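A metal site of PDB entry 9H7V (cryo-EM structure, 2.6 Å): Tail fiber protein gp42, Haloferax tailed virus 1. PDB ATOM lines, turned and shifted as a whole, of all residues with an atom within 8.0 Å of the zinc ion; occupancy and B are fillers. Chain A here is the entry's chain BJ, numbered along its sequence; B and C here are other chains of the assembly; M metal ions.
The zinc ion is bound by a ring nitrogen (NE2) of His 216 of chain B, a ring nitrogen (NE2) of His 216 of chain A and a ring nitrogen (NE2) of His 220 of chain A.
The zinc ion has three donor atoms within binding distance.
NE2 of His 216 of chain C touches the zinc ion, at 3.3 Å.
The nearest printed residue that does not touch the zinc ion is His 220 of chain C (4.4 Å).
A ring nitrogen (ND1) of His 216 of chain C lies within hydrogen-bond range of the backbone carbonyl oxygen (O) of Asp 213 of chain C (2.9 Å).
N of His 216 of chain B lies within hydrogen-bond range of OD2 of Asp 226 of chain A, 3.1 Å away.
NE2 of His 216 of chain C lies close to NE2 of His 216 of chain A (3.3 Å).
The backbone carbonyl oxygen (O) of Asp 213 of chain B sits at hydrogen-bond distance from a ring nitrogen (ND1) of His 216 of chain B (2.7 Å).
O of Asp 226 of chain A sits at hydrogen-bond distance from ND1 of His 220 of chain A (2.8 Å).
The side-chain carboxylate (OD2) of Asp 226 of chain C sits at hydrogen-bond distance from the backbone NH (N) of His 216 of chain A, at 3.1 Å.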
ATOM      1  N   GLU A 212     -15.271 -24.384  14.686  1.00  0.00           N
ATOM      2  CA  GLU A 212     -14.618 -24.755  13.437  1.00  0.00           C
ATOM      3  C   GLU A 212     -14.095 -26.185  13.481  1.00  0.00           C
ATOM      4  O   GLU A 212     -13.489 -26.601  14.481  1.00  0.00           O
ATOM      5  CB  GLU A 212     -13.489 -23.773  13.103  1.00  0.00           C
ATOM      6  CG  GLU A 212     -13.972 -22.378  12.733  1.00  0.00           C
ATOM      7  CD  GLU A 212     -14.510 -22.174  11.324  1.00  0.00           C
ATOM      8  OE1 GLU A 212     -15.287 -23.032  10.843  1.00  0.00           O
ATOM      9  OE2 GLU A 212     -14.147 -21.158  10.708  1.00  0.00           O
ATOM     10  N   ASP A 213     -14.331 -26.930  12.390  1.00  0.00           N
ATOM     11  CA  ASP A 213     -13.865 -28.298  12.183  1.00  0.00           C
ATOM     12  C   ASP A 213     -12.400 -28.280  11.736  1.00  0.00           C
ATOM     13  O   ASP A 213     -11.887 -27.232  11.351  1.00  0.00           O
ATOM     14  CB  ASP A 213     -14.634 -28.997  11.056  1.00  0.00           C
ATOM     15  CG  ASP A 213     -16.148 -29.000  11.210  1.00  0.00           C
ATOM     16  OD1 ASP A 213     -16.636 -29.593  12.191  1.00  0.00           O
ATOM     17  OD2 ASP A 213     -16.826 -28.423  10.342  1.00  0.00           O
ATOM     18  N   HIS A 216     -10.250 -27.048   7.581  1.00  0.00           N
ATOM     19  CA  HIS A 216     -11.100 -25.896   7.312  1.00  0.00           C
ATOM     20  C   HIS A 216     -10.391 -24.875   6.417  1.00  0.00           C
ATOM     21  O   HIS A 216     -11.041 -23.980   5.885  1.00  0.00           O
ATOM     22  CB  HIS A 216     -11.575 -25.265   8.634  1.00  0.00           C
ATOM     23  CG  HIS A 216     -10.583 -24.326   9.247  1.00  0.00           C
ATOM     24  ND1 HIS A 216      -9.307 -24.731   9.579  1.00  0.00           N
ATOM     25  CD2 HIS A 216     -10.675 -23.028   9.586  1.00  0.00           C
ATOM     26  CE1 HIS A 216      -8.655 -23.713  10.096  1.00  0.00           C
ATOM     27  NE2 HIS A 216      -9.465 -22.651  10.106  1.00  0.00           N
ATOM     28  N   GLY A 217      -9.060 -25.016   6.272  1.00  0.00           N
ATOM     29  CA  GLY A 217      -8.181 -24.034   5.651  1.00  0.00           C
ATOM     30  C   GLY A 217      -8.667 -23.498   4.306  1.00  0.00           C
ATOM     31  O   GLY A 217      -8.406 -22.348   3.964  1.00  0.00           O
ATOM     32  N   SER A 218      -9.396 -24.357   3.574  1.00  0.00           N
ATOM     33  CA  SER A 218     -10.033 -24.077   2.286  1.00  0.00           C
ATOM     34  C   SER A 218     -10.720 -22.704   2.272  1.00  0.00           C
ATOM     35  O   SER A 218     -10.635 -21.991   1.276  1.00  0.00           O
ATOM     36  CB  SER A 218     -10.993 -25.180   1.935  1.00  0.00           C
ATOM     37  OG  SER A 218     -11.670 -24.899   0.724  1.00  0.00           O
ATOM     38  N   LYS A 219     -11.391 -22.349   3.383  1.00  0.00           N
ATOM     39  CA  LYS A 219     -12.237 -21.174   3.468  1.00  0.00           C
ATOM     40  C   LYS A 219     -11.419 -19.877   3.430  1.00  0.00           C
ATOM     41  O   LYS A 219     -11.929 -18.838   3.017  1.00  0.00           O
ATOM     42  CB  LYS A 219     -13.186 -21.262   4.666  1.00  0.00           C
ATOM     43  CG  LYS A 219     -12.576 -20.999   6.038  1.00  0.00           C
ATOM     44  CD  LYS A 219     -13.441 -21.466   7.195  1.00  0.00           C
ATOM     45  CE  LYS A 219     -14.777 -20.752   7.294  1.00  0.00           C
ATOM     46  NZ  LYS A 219     -15.649 -21.362   8.336  1.00  0.00           N
ATOM     47  N   HIS A 220     -10.139 -19.940   3.850  1.00  0.00           N
ATOM     48  CA  HIS A 220      -9.295 -18.756   3.964  1.00  0.00           C
ATOM     49  C   HIS A 220      -8.749 -18.321   2.595  1.00  0.00           C
ATOM     50  O   HIS A 220      -8.194 -17.232   2.474  1.00  0.00           O
ATOM     51  CB  HIS A 220      -8.179 -18.964   5.005  1.00  0.00           C
ATOM     52  CG  HIS A 220      -8.641 -19.162   6.411  1.00  0.00           C
ATOM     53  ND1 HIS A 220      -9.367 -18.215   7.099  1.00  0.00           N
ATOM     54  CD2 HIS A 220      -8.467 -20.197   7.263  1.00  0.00           C
ATOM     55  CE1 HIS A 220      -9.640 -18.658   8.313  1.00  0.00           C
ATOM     56  NE2 HIS A 220      -9.088 -19.868   8.434  1.00  0.00           N
ATOM     57  N   SER A 225     -15.263 -17.740   2.742  1.00  0.00           N
ATOM     58  CA  SER A 225     -15.586 -16.921   3.907  1.00  0.00           C
ATOM     59  C   SER A 225     -14.383 -16.885   4.851  1.00  0.00           C
ATOM     60  O   SER A 225     -13.722 -17.903   5.036  1.00  0.00           O
ATOM     61  CB  SER A 225     -16.834 -17.420   4.594  1.00  0.00           C
ATOM     62  OG  SER A 225     -16.681 -18.770   5.006  1.00  0.00           O
ATOM     63  N   ASP A 226     -14.125 -15.701   5.435  1.00  0.00           N
ATOM     64  CA  ASP A 226     -13.018 -15.443   6.349  1.00  0.00           C
ATOM     65  C   ASP A 226     -11.682 -15.460   5.595  1.00  0.00           C
ATOM     66  O   ASP A 226     -10.660 -15.897   6.139  1.00  0.00           O
ATOM     67  CB  ASP A 226     -13.071 -16.308   7.616  1.00  0.00           C
ATOM     68  CG  ASP A 226     -12.258 -15.792   8.783  1.00  0.00           C
ATOM     69  OD1 ASP A 226     -11.942 -14.581   8.812  1.00  0.00           O
ATOM     70  OD2 ASP A 226     -11.938 -16.605   9.678  1.00  0.00           O
ATOM     71  N   ILE A 228      -8.344 -13.967   4.364  1.00  0.00           N
ATOM     72  CA  ILE A 228      -7.401 -13.081   5.044  1.00  0.00           C
ATOM     73  C   ILE A 228      -6.714 -12.166   4.018  1.00  0.00           C
ATOM     74  O   ILE A 228      -6.543 -12.546   2.860  1.00  0.00           O
ATOM     75  CB  ILE A 228      -6.380 -13.857   5.909  1.00  0.00           C
ATOM     76  CG1 ILE A 228      -5.454 -14.764   5.077  1.00  0.00           C
ATOM     77  CG2 ILE A 228      -7.084 -14.626   7.021  1.00  0.00           C
ATOM     78  CD1 ILE A 228      -4.213 -15.243   5.806  1.00  0.00           C
ATOM     79  N   GLU B 212     -11.904 -22.371  18.344  1.00  0.00           N
ATOM     80  CA  GLU B 212     -11.978 -21.222  17.458  1.00  0.00           C
ATOM     81  C   GLU B 212     -13.344 -21.131  16.776  1.00  0.00           C
ATOM     82  O   GLU B 212     -13.823 -22.105  16.210  1.00  0.00           O
ATOM     83  CB  GLU B 212     -10.850 -21.244  16.423  1.00  0.00           C
ATOM     84  CG  GLU B 212      -9.476 -20.935  17.008  1.00  0.00           C
ATOM     85  CD  GLU B 212      -9.130 -19.473  17.283  1.00  0.00           C
ATOM     86  OE1 GLU B 212     -10.047 -18.689  17.604  1.00  0.00           O
ATOM     87  OE2 GLU B 212      -7.940 -19.129  17.176  1.00  0.00           O
ATOM     88  N   ASP B 213     -13.934 -19.924  16.824  1.00  0.00           N
ATOM     89  CA  ASP B 213     -15.180 -19.576  16.160  1.00  0.00           C
ATOM     90  C   ASP B 213     -14.949 -19.433  14.660  1.00  0.00           C
ATOM     91  O   ASP B 213     -13.816 -19.484  14.194  1.00  0.00           O
ATOM     92  CB  ASP B 213     -15.720 -18.224  16.646  1.00  0.00           C
ATOM     93  CG  ASP B 213     -15.638 -17.979  18.137  1.00  0.00           C
ATOM     94  OD1 ASP B 213     -16.529 -18.454  18.858  1.00  0.00           O
ATOM     95  OD2 ASP B 213     -14.677 -17.299  18.568  1.00  0.00           O
ATOM     96  N   ILE B 214     -16.039 -19.223  13.901  1.00  0.00           N
ATOM     97  CA  ILE B 214     -15.981 -18.624  12.571  1.00  0.00           C
ATOM     98  C   ILE B 214     -15.489 -17.185  12.720  1.00  0.00           C
ATOM     99  O   ILE B 214     -15.611 -16.592  13.791  1.00  0.00           O
ATOM    100  CB  ILE B 214     -17.344 -18.693  11.848  1.00  0.00           C
ATOM    101  CG1 ILE B 214     -18.454 -17.956  12.601  1.00  0.00           C
ATOM    102  CG2 ILE B 214     -17.727 -20.134  11.532  1.00  0.00           C
ATOM    103  CD1 ILE B 214     -19.584 -17.444  11.728  1.00  0.00           C
ATOM    104  N   ASN B 215     -14.923 -16.628  11.623  1.00  0.00           N
ATOM    105  CA  ASN B 215     -14.470 -15.245  11.531  1.00  0.00           C
ATOM    106  C   ASN B 215     -13.265 -14.983  12.432  1.00  0.00           C
ATOM    107  O   ASN B 215     -13.068 -13.864  12.903  1.00  0.00           O
ATOM    108  CB  ASN B 215     -15.607 -14.224  11.731  1.00  0.00           C
ATOM    109  CG  ASN B 215     -16.813 -14.455  10.835  1.00  0.00           C
ATOM    110  OD1 ASN B 215     -16.693 -14.935   9.712  1.00  0.00           O
ATOM    111  ND2 ASN B 215     -17.988 -14.096  11.330  1.00  0.00           N
ATOM    112  N   HIS B 216     -12.439 -16.026  12.632  1.00  0.00           N
ATOM    113  CA  HIS B 216     -11.243 -15.949  13.467  1.00  0.00           C
ATOM    114  C   HIS B 216     -10.070 -15.337  12.706  1.00  0.00           C
ATOM    115  O   HIS B 216      -9.239 -14.648  13.304  1.00  0.00           O
ATOM    116  CB  HIS B 216     -10.880 -17.345  13.995  1.00  0.00           C
ATOM    117  CG  HIS B 216     -10.688 -18.352  12.913  1.00  0.00           C
ATOM    118  ND1 HIS B 216     -11.744 -19.109  12.426  1.00  0.00           N
ATOM    119  CD2 HIS B 216      -9.602 -18.715  12.204  1.00  0.00           C
ATOM    120  CE1 HIS B 216     -11.304 -19.902  11.467  1.00  0.00           C
ATOM    121  NE2 HIS B 216      -9.992 -19.679  11.317  1.00  0.00           N
ATOM    122  N   GLY B 217     -10.031 -15.564  11.381  1.00  0.00           N
ATOM    123  CA  GLY B 217      -8.871 -15.369  10.516  1.00  0.00           C
ATOM    124  C   GLY B 217      -8.224 -13.982  10.595  1.00  0.00           C
ATOM    125  O   GLY B 217      -7.053 -13.832  10.270  1.00  0.00           O
ATOM    126  N   SER B 218      -9.016 -12.985  11.024  1.00  0.00           N
ATOM    127  CA  SER B 218      -8.576 -11.603  11.221  1.00  0.00           C
ATOM    128  C   SER B 218      -7.395 -11.515  12.178  1.00  0.00           C
ATOM    129  O   SER B 218      -6.632 -10.550  12.128  1.00  0.00           O
ATOM    130  CB  SER B 218      -9.729 -10.748  11.690  1.00  0.00           C
ATOM    131  OG  SER B 218      -9.343  -9.379  11.773  1.00  0.00           O
ATOM    132  N   LYS B 219      -7.240 -12.540  13.041  1.00  0.00           N
ATOM    133  CA  LYS B 219      -6.150 -12.643  13.994  1.00  0.00           C
ATOM    134  C   LYS B 219      -4.805 -12.754  13.278  1.00  0.00           C
ATOM    135  O   LYS B 219      -3.805 -12.241  13.787  1.00  0.00           O
ATOM    136  CB  LYS B 219      -6.399 -13.810  14.964  1.00  0.00           C
ATOM    137  CG  LYS B 219      -6.303 -15.214  14.378  1.00  0.00           C
ATOM    138  CD  LYS B 219      -6.686 -16.309  15.350  1.00  0.00           C
ATOM    139  CE  LYS B 219      -5.653 -16.512  16.452  1.00  0.00           C
ATOM    140  NZ  LYS B 219      -6.271 -17.058  17.687  1.00  0.00           N
ATOM    141  N   HIS B 220      -4.784 -13.402  12.107  1.00  0.00           N
ATOM    142  CA  HIS B 220      -3.559 -13.727  11.385  1.00  0.00           C
ATOM    143  C   HIS B 220      -2.930 -12.484  10.734  1.00  0.00           C
ATOM    144  O   HIS B 220      -1.898 -12.595  10.086  1.00  0.00           O
ATOM    145  CB  HIS B 220      -3.802 -14.842  10.334  1.00  0.00           C
ATOM    146  CG  HIS B 220      -4.442 -16.107  10.816  1.00  0.00           C
ATOM    147  ND1 HIS B 220      -3.882 -16.921  11.774  1.00  0.00           N
ATOM    148  CD2 HIS B 220      -5.583 -16.721  10.425  1.00  0.00           C
ATOM    149  CE1 HIS B 220      -4.661 -17.971  11.976  1.00  0.00           C
ATOM    150  NE2 HIS B 220      -5.711 -17.871  11.161  1.00  0.00           N
ATOM    151  N   GLU C 212     -11.058 -27.592  16.004  1.00  0.00           N
ATOM    152  CA  GLU C 212      -9.878 -26.747  15.854  1.00  0.00           C
ATOM    153  C   GLU C 212      -9.625 -25.910  17.110  1.00  0.00           C
ATOM    154  O   GLU C 212     -10.491 -25.168  17.566  1.00  0.00           O
ATOM    155  CB  GLU C 212      -9.955 -25.879  14.601  1.00  0.00           C
ATOM    156  CG  GLU C 212      -9.611 -26.615  13.316  1.00  0.00           C
ATOM    157  CD  GLU C 212      -8.165 -26.986  13.036  1.00  0.00           C
ATOM    158  OE1 GLU C 212      -7.336 -26.959  13.976  1.00  0.00           O
ATOM    159  OE2 GLU C 212      -7.856 -27.317  11.873  1.00  0.00           O
ATOM    160  N   ASP C 213      -8.390 -26.041  17.620  1.00  0.00           N
ATOM    161  CA  ASP C 213      -7.843 -25.316  18.759  1.00  0.00           C
ATOM    162  C   ASP C 213      -7.476 -23.899  18.333  1.00  0.00           C
ATOM    163  O   ASP C 213      -7.516 -23.576  17.148  1.00  0.00           O
ATOM    164  CB  ASP C 213      -6.587 -26.013  19.292  1.00  0.00           C
ATOM    165  CG  ASP C 213      -6.656 -27.531  19.261  1.00  0.00           C
ATOM    166  OD1 ASP C 213      -6.993 -28.110  20.314  1.00  0.00           O
ATOM    167  OD2 ASP C 213      -6.360 -28.117  18.209  1.00  0.00           O
ATOM    168  N   HIS C 216      -3.981 -22.433  15.365  1.00  0.00           N
ATOM    169  CA  HIS C 216      -3.816 -23.630  14.537  1.00  0.00           C
ATOM    170  C   HIS C 216      -3.062 -23.330  13.240  1.00  0.00           C
ATOM    171  O   HIS C 216      -2.652 -24.251  12.545  1.00  0.00           O
ATOM    172  CB  HIS C 216      -5.187 -24.243  14.245  1.00  0.00           C
ATOM    173  CG  HIS C 216      -6.168 -23.266  13.687  1.00  0.00           C
ATOM    174  ND1 HIS C 216      -7.207 -22.738  14.440  1.00  0.00           N
ATOM    175  CD2 HIS C 216      -6.265 -22.688  12.472  1.00  0.00           C
ATOM    176  CE1 HIS C 216      -7.901 -21.893  13.708  1.00  0.00           C
ATOM    177  NE2 HIS C 216      -7.345 -21.847  12.494  1.00  0.00           N
ATOM    178  N   GLY C 217      -2.854 -22.034  12.938  1.00  0.00           N
ATOM    179  CA  GLY C 217      -2.371 -21.549  11.649  1.00  0.00           C
ATOM    180  C   GLY C 217      -1.048 -22.166  11.186  1.00  0.00           C
ATOM    181  O   GLY C 217      -0.779 -22.201   9.981  1.00  0.00           O
ATOM    182  N   HIS C 220      -1.126 -24.738   8.434  1.00  0.00           N
ATOM    183  CA  HIS C 220      -1.467 -24.284   7.087  1.00  0.00           C
ATOM    184  C   HIS C 220      -0.218 -24.040   6.233  1.00  0.00           C
ATOM    185  O   HIS C 220      -0.333 -23.900   5.022  1.00  0.00           O
ATOM    186  CB  HIS C 220      -2.344 -23.017   7.127  1.00  0.00           C
ATOM    187  CG  HIS C 220      -3.674 -23.126   7.802  1.00  0.00           C
ATOM    188  ND1 HIS C 220      -4.490 -24.236   7.691  1.00  0.00           N
ATOM    189  CD2 HIS C 220      -4.370 -22.230   8.536  1.00  0.00           C
ATOM    190  CE1 HIS C 220      -5.614 -24.035   8.363  1.00  0.00           C
ATOM    191  NE2 HIS C 220      -5.557 -22.804   8.892  1.00  0.00           N
ATOM    192  N   ASP C 226      -3.805 -29.787   5.843  1.00  0.00           N
ATOM    193  CA  ASP C 226      -4.678 -28.622   5.718  1.00  0.00           C
ATOM    194  C   ASP C 226      -3.873 -27.378   5.333  1.00  0.00           C
ATOM    195  O   ASP C 226      -3.949 -26.347   5.997  1.00  0.00           O
ATOM    196  CB  ASP C 226      -5.620 -28.454   6.917  1.00  0.00           C
ATOM    197  CG  ASP C 226      -6.750 -27.458   6.691  1.00  0.00           C
ATOM    198  OD1 ASP C 226      -7.193 -27.314   5.528  1.00  0.00           O
ATOM    199  OD2 ASP C 226      -7.189 -26.835   7.672  1.00  0.00           O
ATOM    200  N   ILE C 228      -2.942 -24.169   2.806  1.00  0.00           N
ATOM    201  CA  ILE C 228      -3.761 -23.185   2.103  1.00  0.00           C
ATOM    202  C   ILE C 228      -3.020 -22.639   0.875  1.00  0.00           C
ATOM    203  O   ILE C 228      -1.813 -22.440   0.916  1.00  0.00           O
ATOM    204  CB  ILE C 228      -4.260 -22.053   3.046  1.00  0.00           C
ATOM    205  CG1 ILE C 228      -3.124 -21.169   3.581  1.00  0.00           C
ATOM    206  CG2 ILE C 228      -5.103 -22.636   4.171  1.00  0.00           C
ATOM    207  CD1 ILE C 228      -3.589 -19.914   4.291  1.00  0.00           C
HETATM  208 ZN    ZN M   1      -9.314 -20.795  10.052  1.00  0.00          ZN
